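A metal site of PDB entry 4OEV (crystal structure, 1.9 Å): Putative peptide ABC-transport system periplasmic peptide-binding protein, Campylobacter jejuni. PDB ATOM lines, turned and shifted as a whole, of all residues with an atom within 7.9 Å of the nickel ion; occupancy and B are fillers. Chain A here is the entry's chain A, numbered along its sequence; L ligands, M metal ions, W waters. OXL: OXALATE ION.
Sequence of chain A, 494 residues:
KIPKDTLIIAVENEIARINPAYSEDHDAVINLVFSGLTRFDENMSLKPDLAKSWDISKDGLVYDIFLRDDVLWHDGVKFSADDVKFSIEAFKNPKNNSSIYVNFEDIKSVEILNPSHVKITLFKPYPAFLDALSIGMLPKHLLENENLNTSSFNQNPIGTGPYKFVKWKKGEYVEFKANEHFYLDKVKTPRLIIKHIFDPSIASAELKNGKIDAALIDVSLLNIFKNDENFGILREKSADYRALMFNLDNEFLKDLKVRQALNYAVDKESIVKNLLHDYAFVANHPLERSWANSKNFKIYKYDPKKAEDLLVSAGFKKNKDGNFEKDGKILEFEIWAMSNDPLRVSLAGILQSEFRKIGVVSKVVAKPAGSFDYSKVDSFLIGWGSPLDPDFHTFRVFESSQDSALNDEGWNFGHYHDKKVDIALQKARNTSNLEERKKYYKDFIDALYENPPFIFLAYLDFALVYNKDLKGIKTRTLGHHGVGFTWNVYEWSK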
ATOM      1  N   GLU A  12      23.382   7.355   0.068  1.00  0.00           N
ATOM      2  CA  GLU A  12      23.201   6.357   1.173  1.00  0.00           C
ATOM      3  C   GLU A  12      22.037   5.353   0.943  1.00  0.00           C
ATOM      4  O   GLU A  12      22.220   4.127   1.088  1.00  0.00           O
ATOM      5  CB  GLU A  12      23.007   7.072   2.480  1.00  0.00           C
ATOM      6  CG  GLU A  12      22.875   6.131   3.708  1.00  0.00           C
ATOM      7  CD  GLU A  12      22.467   6.871   4.924  1.00  0.00           C
ATOM      8  OE1 GLU A  12      22.286   8.103   4.796  1.00  0.00           O
ATOM      9  OE2 GLU A  12      22.308   6.245   6.004  1.00  0.00           O
ATOM     10  N   ASN A  13      20.867   5.879   0.532  1.00  0.00           N
ATOM     11  CA  ASN A  13      19.640   5.098   0.412  1.00  0.00           C
ATOM     12  C   ASN A  13      19.240   4.927  -1.042  1.00  0.00           C
ATOM     13  O   ASN A  13      19.560   5.769  -1.880  1.00  0.00           O
ATOM     14  CB  ASN A  13      18.516   5.802   1.169  1.00  0.00           C
ATOM     15  CG  ASN A  13      18.835   5.978   2.620  1.00  0.00           C
ATOM     16  OD1 ASN A  13      18.801   5.008   3.376  1.00  0.00           O
ATOM     17  ND2 ASN A  13      19.157   7.210   3.031  1.00  0.00           N
ATOM     18  N   GLU A  24       9.660   8.010  -0.412  1.00  0.00           N
ATOM     19  CA  GLU A  24       9.738   8.102   1.039  1.00  0.00           C
ATOM     20  C   GLU A  24      10.756   9.156   1.485  1.00  0.00           C
ATOM     21  O   GLU A  24      11.243   9.089   2.606  1.00  0.00           O
ATOM     22  CB  GLU A  24      10.091   6.751   1.669  1.00  0.00           C
ATOM     23  CG  GLU A  24       8.939   5.754   1.515  1.00  0.00           C
ATOM     24  CD  GLU A  24       9.095   4.532   2.367  1.00  0.00           C
ATOM     25  OE1 GLU A  24      10.213   3.956   2.422  1.00  0.00           O
ATOM     26  OE2 GLU A  24       8.125   4.168   3.054  1.00  0.00           O
ATOM     27  N   ASP A  25      11.055  10.090   0.592  1.00  0.00           N
ATOM     28  CA  ASP A  25      12.008  11.195   0.817  1.00  0.00           C
ATOM     29  C   ASP A  25      13.392  10.646   1.190  1.00  0.00           C
ATOM     30  O   ASP A  25      14.169  11.333   1.868  1.00  0.00           O
ATOM     31  CB  ASP A  25      11.549  12.171   1.925  1.00  0.00           C
ATOM     32  CG  ASP A  25      10.328  12.990   1.547  1.00  0.00           C
ATOM     33  OD1 ASP A  25       9.929  12.979   0.366  1.00  0.00           O
ATOM     34  OD2 ASP A  25       9.774  13.698   2.427  1.00  0.00           O
ATOM     35  N   HIS A  26      13.723   9.432   0.759  1.00  0.00           N
ATOM     36  CA  HIS A  26      15.050   8.895   1.057  1.00  0.00           C
ATOM     37  C   HIS A  26      15.977   8.763  -0.137  1.00  0.00           C
ATOM     38  O   HIS A  26      17.166   8.580   0.027  1.00  0.00           O
ATOM     39  CB  HIS A  26      14.960   7.515   1.695  1.00  0.00           C
ATOM     40  CG  HIS A  26      14.691   7.555   3.151  1.00  0.00           C
ATOM     41  ND1 HIS A  26      13.455   7.900   3.667  1.00  0.00           N
ATOM     42  CD2 HIS A  26      15.511   7.357   4.210  1.00  0.00           C
ATOM     43  CE1 HIS A  26      13.527   7.877   4.991  1.00  0.00           C
ATOM     44  NE2 HIS A  26      14.764   7.572   5.332  1.00  0.00           N
ATOM     45  N   ASP A 240      17.456  18.191   9.051  1.00  0.00           N
ATOM     46  CA  ASP A 240      17.559  16.818   9.506  1.00  0.00           C
ATOM     47  C   ASP A 240      17.998  16.722  10.970  1.00  0.00           C
ATOM     48  O   ASP A 240      19.037  17.268  11.325  1.00  0.00           O
ATOM     49  CB  ASP A 240      18.574  16.081   8.632  1.00  0.00           C
ATOM     50  CG  ASP A 240      18.538  14.588   8.849  1.00  0.00           C
ATOM     51  OD1 ASP A 240      17.594  14.085   9.485  1.00  0.00           O
ATOM     52  OD2 ASP A 240      19.430  13.910   8.326  1.00  0.00           O
ATOM     53  N   ARG A 242      18.665  14.092  14.650  1.00  0.00           N
ATOM     54  CA  ARG A 242      18.808  12.761  15.203  1.00  0.00           C
ATOM     55  C   ARG A 242      18.170  12.765  16.588  1.00  0.00           C
ATOM     56  O   ARG A 242      18.192  13.764  17.259  1.00  0.00           O
ATOM     57  CB  ARG A 242      20.293  12.311  15.351  1.00  0.00           C
ATOM     58  CG  ARG A 242      20.987  12.144  13.990  1.00  0.00           C
ATOM     59  CD  ARG A 242      20.568  10.882  13.279  1.00  0.00           C
ATOM     60  NE  ARG A 242      20.949  10.938  11.877  1.00  0.00           N
ATOM     61  CZ  ARG A 242      20.241  11.535  10.919  1.00  0.00           C
ATOM     62  NH1 ARG A 242      19.086  12.143  11.187  1.00  0.00           N
ATOM     63  NH2 ARG A 242      20.695  11.527   9.686  1.00  0.00           N
ATOM     64  N   MET A 338      21.769   1.961  13.415  1.00  0.00           N
ATOM     65  CA  MET A 338      22.278   1.534  12.114  1.00  0.00           C
ATOM     66  C   MET A 338      23.797   1.405  12.172  1.00  0.00           C
ATOM     67  O   MET A 338      24.477   2.415  12.333  1.00  0.00           O
ATOM     68  CB  MET A 338      21.896   2.568  11.050  1.00  0.00           C
ATOM     69  CG  MET A 338      20.386   2.803  10.874  1.00  0.00           C
ATOM     70  SD  MET A 338      20.222   4.101   9.683  1.00  0.00           S
ATOM     71  CE  MET A 338      18.427   4.243   9.461  1.00  0.00           C
ATOM     72  N   ARG A 344      25.381   7.451  14.367  1.00  0.00           N
ATOM     73  CA  ARG A 344      24.330   6.826  15.175  1.00  0.00           C
ATOM     74  C   ARG A 344      24.910   5.811  16.142  1.00  0.00           C
ATOM     75  O   ARG A 344      24.457   5.720  17.296  1.00  0.00           O
ATOM     76  CB  ARG A 344      23.272   6.174  14.271  1.00  0.00           C
ATOM     77  CG  ARG A 344      22.765   7.107  13.192  1.00  0.00           C
ATOM     78  CD  ARG A 344      21.437   6.609  12.664  1.00  0.00           C
ATOM     79  NE  ARG A 344      21.000   7.223  11.388  1.00  0.00           N
ATOM     80  CZ  ARG A 344      19.710   7.387  11.042  1.00  0.00           C
ATOM     81  NH1 ARG A 344      19.382   7.895   9.851  1.00  0.00           N
ATOM     82  NH2 ARG A 344      18.737   7.082  11.894  1.00  0.00           N
ATOM     83  N   TYR A 374      12.581  -1.483  12.438  1.00  0.00           N
ATOM     84  CA  TYR A 374      12.818  -0.391  13.352  1.00  0.00           C
ATOM     85  C   TYR A 374      11.677  -0.154  14.345  1.00  0.00           C
ATOM     86  O   TYR A 374      11.871   0.522  15.343  1.00  0.00           O
ATOM     87  CB  TYR A 374      13.089   0.905  12.601  1.00  0.00           C
ATOM     88  CG  TYR A 374      14.203   0.861  11.565  1.00  0.00           C
ATOM     89  CD1 TYR A 374      14.221   1.762  10.485  1.00  0.00           C
ATOM     90  CD2 TYR A 374      15.232  -0.089  11.636  1.00  0.00           C
ATOM     91  CE1 TYR A 374      15.218   1.707   9.515  1.00  0.00           C
ATOM     92  CE2 TYR A 374      16.212  -0.155  10.689  1.00  0.00           C
ATOM     93  CZ  TYR A 374      16.224   0.763   9.624  1.00  0.00           C
ATOM     94  OH  TYR A 374      17.238   0.695   8.661  1.00  0.00           O
ATOM     95  N   PHE A 380      15.484   3.275  19.276  1.00  0.00           N
ATOM     96  CA  PHE A 380      16.128   3.321  17.967  1.00  0.00           C
ATOM     97  C   PHE A 380      16.719   4.713  17.742  1.00  0.00           C
ATOM     98  O   PHE A 380      16.047   5.699  18.017  1.00  0.00           O
ATOM     99  CB  PHE A 380      15.085   2.978  16.851  1.00  0.00           C
ATOM    100  CG  PHE A 380      15.650   2.969  15.465  1.00  0.00           C
ATOM    101  CD1 PHE A 380      16.448   1.916  15.019  1.00  0.00           C
ATOM    102  CD2 PHE A 380      15.356   4.010  14.582  1.00  0.00           C
ATOM    103  CE1 PHE A 380      16.956   1.913  13.722  1.00  0.00           C
ATOM    104  CE2 PHE A 380      15.867   4.015  13.265  1.00  0.00           C
ATOM    105  CZ  PHE A 380      16.681   2.983  12.853  1.00  0.00           C
ATOM    106  N   ILE A 382      17.036   7.313  15.681  1.00  0.00           N
ATOM    107  CA  ILE A 382      16.171   7.650  14.519  1.00  0.00           C
ATOM    108  C   ILE A 382      16.520   9.042  13.965  1.00  0.00           C
ATOM    109  O   ILE A 382      17.260   9.783  14.602  1.00  0.00           O
ATOM    110  CB  ILE A 382      14.680   7.632  14.976  1.00  0.00           C
ATOM    111  CG1 ILE A 382      13.687   7.504  13.777  1.00  0.00           C
ATOM    112  CG2 ILE A 382      14.359   8.993  15.720  1.00  0.00           C
ATOM    113  CD1 ILE A 382      12.294   7.100  14.237  1.00  0.00           C
ATOM    114  N   GLY A 383      15.998   9.421  12.766  1.00  0.00           N
ATOM    115  CA  GLY A 383      16.272  10.743  12.273  1.00  0.00           C
ATOM    116  C   GLY A 383      15.061  11.081  11.330  1.00  0.00           C
ATOM    117  O   GLY A 383      14.465  10.129  10.813  1.00  0.00           O
ATOM    118  N   TRP A 384      14.688  12.357  11.211  1.00  0.00           N
ATOM    119  CA  TRP A 384      13.648  12.826  10.237  1.00  0.00           C
ATOM    120  C   TRP A 384      13.934  14.267   9.956  1.00  0.00           C
ATOM    121  O   TRP A 384      14.771  14.850  10.610  1.00  0.00           O
ATOM    122  CB  TRP A 384      12.199  12.724  10.794  1.00  0.00           C
ATOM    123  CG  TRP A 384      11.731  11.365  11.133  1.00  0.00           C
ATOM    124  CD1 TRP A 384      11.478  10.866  12.405  1.00  0.00           C
ATOM    125  CD2 TRP A 384      11.473  10.323  10.225  1.00  0.00           C
ATOM    126  NE1 TRP A 384      11.083   9.549  12.309  1.00  0.00           N
ATOM    127  CE2 TRP A 384      11.047   9.205  10.977  1.00  0.00           C
ATOM    128  CE3 TRP A 384      11.500  10.220   8.830  1.00  0.00           C
ATOM    129  CZ2 TRP A 384      10.689   7.997  10.370  1.00  0.00           C
ATOM    130  CZ3 TRP A 384      11.158   9.018   8.237  1.00  0.00           C
ATOM    131  CH2 TRP A 384      10.737   7.937   9.008  1.00  0.00           C
ATOM    132  N   GLY A 385      13.217  14.874   8.996  1.00  0.00           N
ATOM    133  CA  GLY A 385      13.345  16.309   8.847  1.00  0.00           C
ATOM    134  C   GLY A 385      13.219  16.748   7.385  1.00  0.00           C
ATOM    135  O   GLY A 385      13.772  16.094   6.501  1.00  0.00           O
ATOM    136  N   HIS A 393       7.170  16.023   7.517  1.00  0.00           N
ATOM    137  CA  HIS A 393       7.744  14.995   8.398  1.00  0.00           C
ATOM    138  C   HIS A 393       7.127  15.087   9.808  1.00  0.00           C
ATOM    139  O   HIS A 393       7.736  14.714  10.801  1.00  0.00           O
ATOM    140  CB  HIS A 393       9.277  15.099   8.432  1.00  0.00           C
ATOM    141  CG  HIS A 393       9.916  14.579   7.186  1.00  0.00           C
ATOM    142  ND1 HIS A 393      11.177  14.024   7.157  1.00  0.00           N
ATOM    143  CD2 HIS A 393       9.442  14.486   5.917  1.00  0.00           C
ATOM    144  CE1 HIS A 393      11.470  13.662   5.923  1.00  0.00           C
ATOM    145  NE2 HIS A 393      10.419  13.899   5.155  1.00  0.00           N
ATOM    146  N   PHE A 413       7.001   4.911  14.024  1.00  0.00           N
ATOM    147  CA  PHE A 413       7.545   3.635  14.303  1.00  0.00           C
ATOM    148  C   PHE A 413       7.577   3.282  15.799  1.00  0.00           C
ATOM    149  O   PHE A 413       7.731   2.092  16.107  1.00  0.00           O
ATOM    150  CB  PHE A 413       8.961   3.523  13.712  1.00  0.00           C
ATOM    151  CG  PHE A 413       8.998   3.598  12.177  1.00  0.00           C
ATOM    152  CD1 PHE A 413       7.891   3.250  11.454  1.00  0.00           C
ATOM    153  CD2 PHE A 413      10.153   3.897  11.505  1.00  0.00           C
ATOM    154  CE1 PHE A 413       7.913   3.306  10.030  1.00  0.00           C
ATOM    155  CE2 PHE A 413      10.174   3.926  10.095  1.00  0.00           C
ATOM    156  CZ  PHE A 413       9.077   3.628   9.386  1.00  0.00           C
ATOM    157  N   HIS A 480      16.316  15.216   5.480  1.00  0.00           N
ATOM    158  CA  HIS A 480      16.709  13.968   6.129  1.00  0.00           C
ATOM    159  C   HIS A 480      17.626  13.147   5.202  1.00  0.00           C
ATOM    160  O   HIS A 480      17.353  13.029   3.989  1.00  0.00           O
ATOM    161  CB  HIS A 480      15.436  13.239   6.515  1.00  0.00           C
ATOM    162  CG  HIS A 480      15.663  11.911   7.142  1.00  0.00           C
ATOM    163  ND1 HIS A 480      16.526  11.733   8.214  1.00  0.00           N
ATOM    164  CD2 HIS A 480      15.136  10.699   6.866  1.00  0.00           C
ATOM    165  CE1 HIS A 480      16.524  10.463   8.559  1.00  0.00           C
ATOM    166  NE2 HIS A 480      15.683   9.806   7.782  1.00  0.00           N
ATOM    167  N   HIS A 481      18.741  12.679   5.766  1.00  0.00           N
ATOM    168  CA  HIS A 481      19.858  12.002   5.080  1.00  0.00           C
ATOM    169  C   HIS A 481      20.565  12.898   4.087  1.00  0.00           C
ATOM    170  O   HIS A 481      21.303  12.387   3.264  1.00  0.00           O
ATOM    171  CB  HIS A 481      19.454  10.709   4.339  1.00  0.00           C
ATOM    172  CG  HIS A 481      18.925   9.616   5.237  1.00  0.00           C
ATOM    173  ND1 HIS A 481      19.740   8.799   5.999  1.00  0.00           N
ATOM    174  CD2 HIS A 481      17.653   9.192   5.451  1.00  0.00           C
ATOM    175  CE1 HIS A 481      18.989   7.931   6.661  1.00  0.00           C
ATOM    176  NE2 HIS A 481      17.716   8.152   6.338  1.00  0.00           N
HETATM  177  C1  OXL L   1      15.808   7.090  10.005  1.00  0.00           C
HETATM  178  C2  OXL L   1      14.417   6.888   9.437  1.00  0.00           C
HETATM  179  O1  OXL L   1      16.104   6.956  11.274  1.00  0.00           O
HETATM  180  O2  OXL L   1      13.681   6.086  10.035  1.00  0.00           O
HETATM  181  O3  OXL L   1      16.703   7.350   9.171  1.00  0.00           O
HETATM  182  O4  OXL L   1      14.048   7.392   8.308  1.00  0.00           O
HETATM  183 NI    NI M   1      15.787   7.774   7.295  1.00  0.00          NI
HETATM  184  O   HOH W   1      15.997   5.874   6.821  1.00  0.00           O
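The backbone carbonyl oxygen of Gly 383 sits close to a ring nitrogen (NE2) of His 480 (3.3 Å). A ring nitrogen (ND1) of His 480 lies within hydrogen-bond range of the side-chain carboxylate (OD1) of Asp 240. The backbone NH (N) of His 480 sits at hydrogen-bond distance from the backbone carbonyl oxygen (O) of Gly 385, 2.9 Å away. A ring nitrogen (ND1) of His 481 sits close to the side-chain amide nitrogen (ND2) of Asn 13, at 3.4 Å. OE1 of Glu 12 lies within hydrogen-bond range of ND1 of His 481 (2.9 Å). The side-chain carboxylate (OD2) of Asp 240 lies within hydrogen-bond range of the backbone NH (N) of His 481, 2.9 Å away. ND1 of His 26 is in hydrogen-bond range of O of Glu 24 (2.7 Å).
Three residues have an atom within 4 Å of the nickel ion: His 26, His 480 and His 481. The nearest printed residue that does not touch the nickel ion is Arg 344 (4.4 Å).
The nickel ion is bound by water W1 (2.0 Å), O4 of the ligand (2.0 Å), NE2 of His 480 (2.1 Å), O3 of the ligand (2.1 Å), NE2 of His 481 (2.2 Å) and NE2 of His 26 (2.2 Å).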
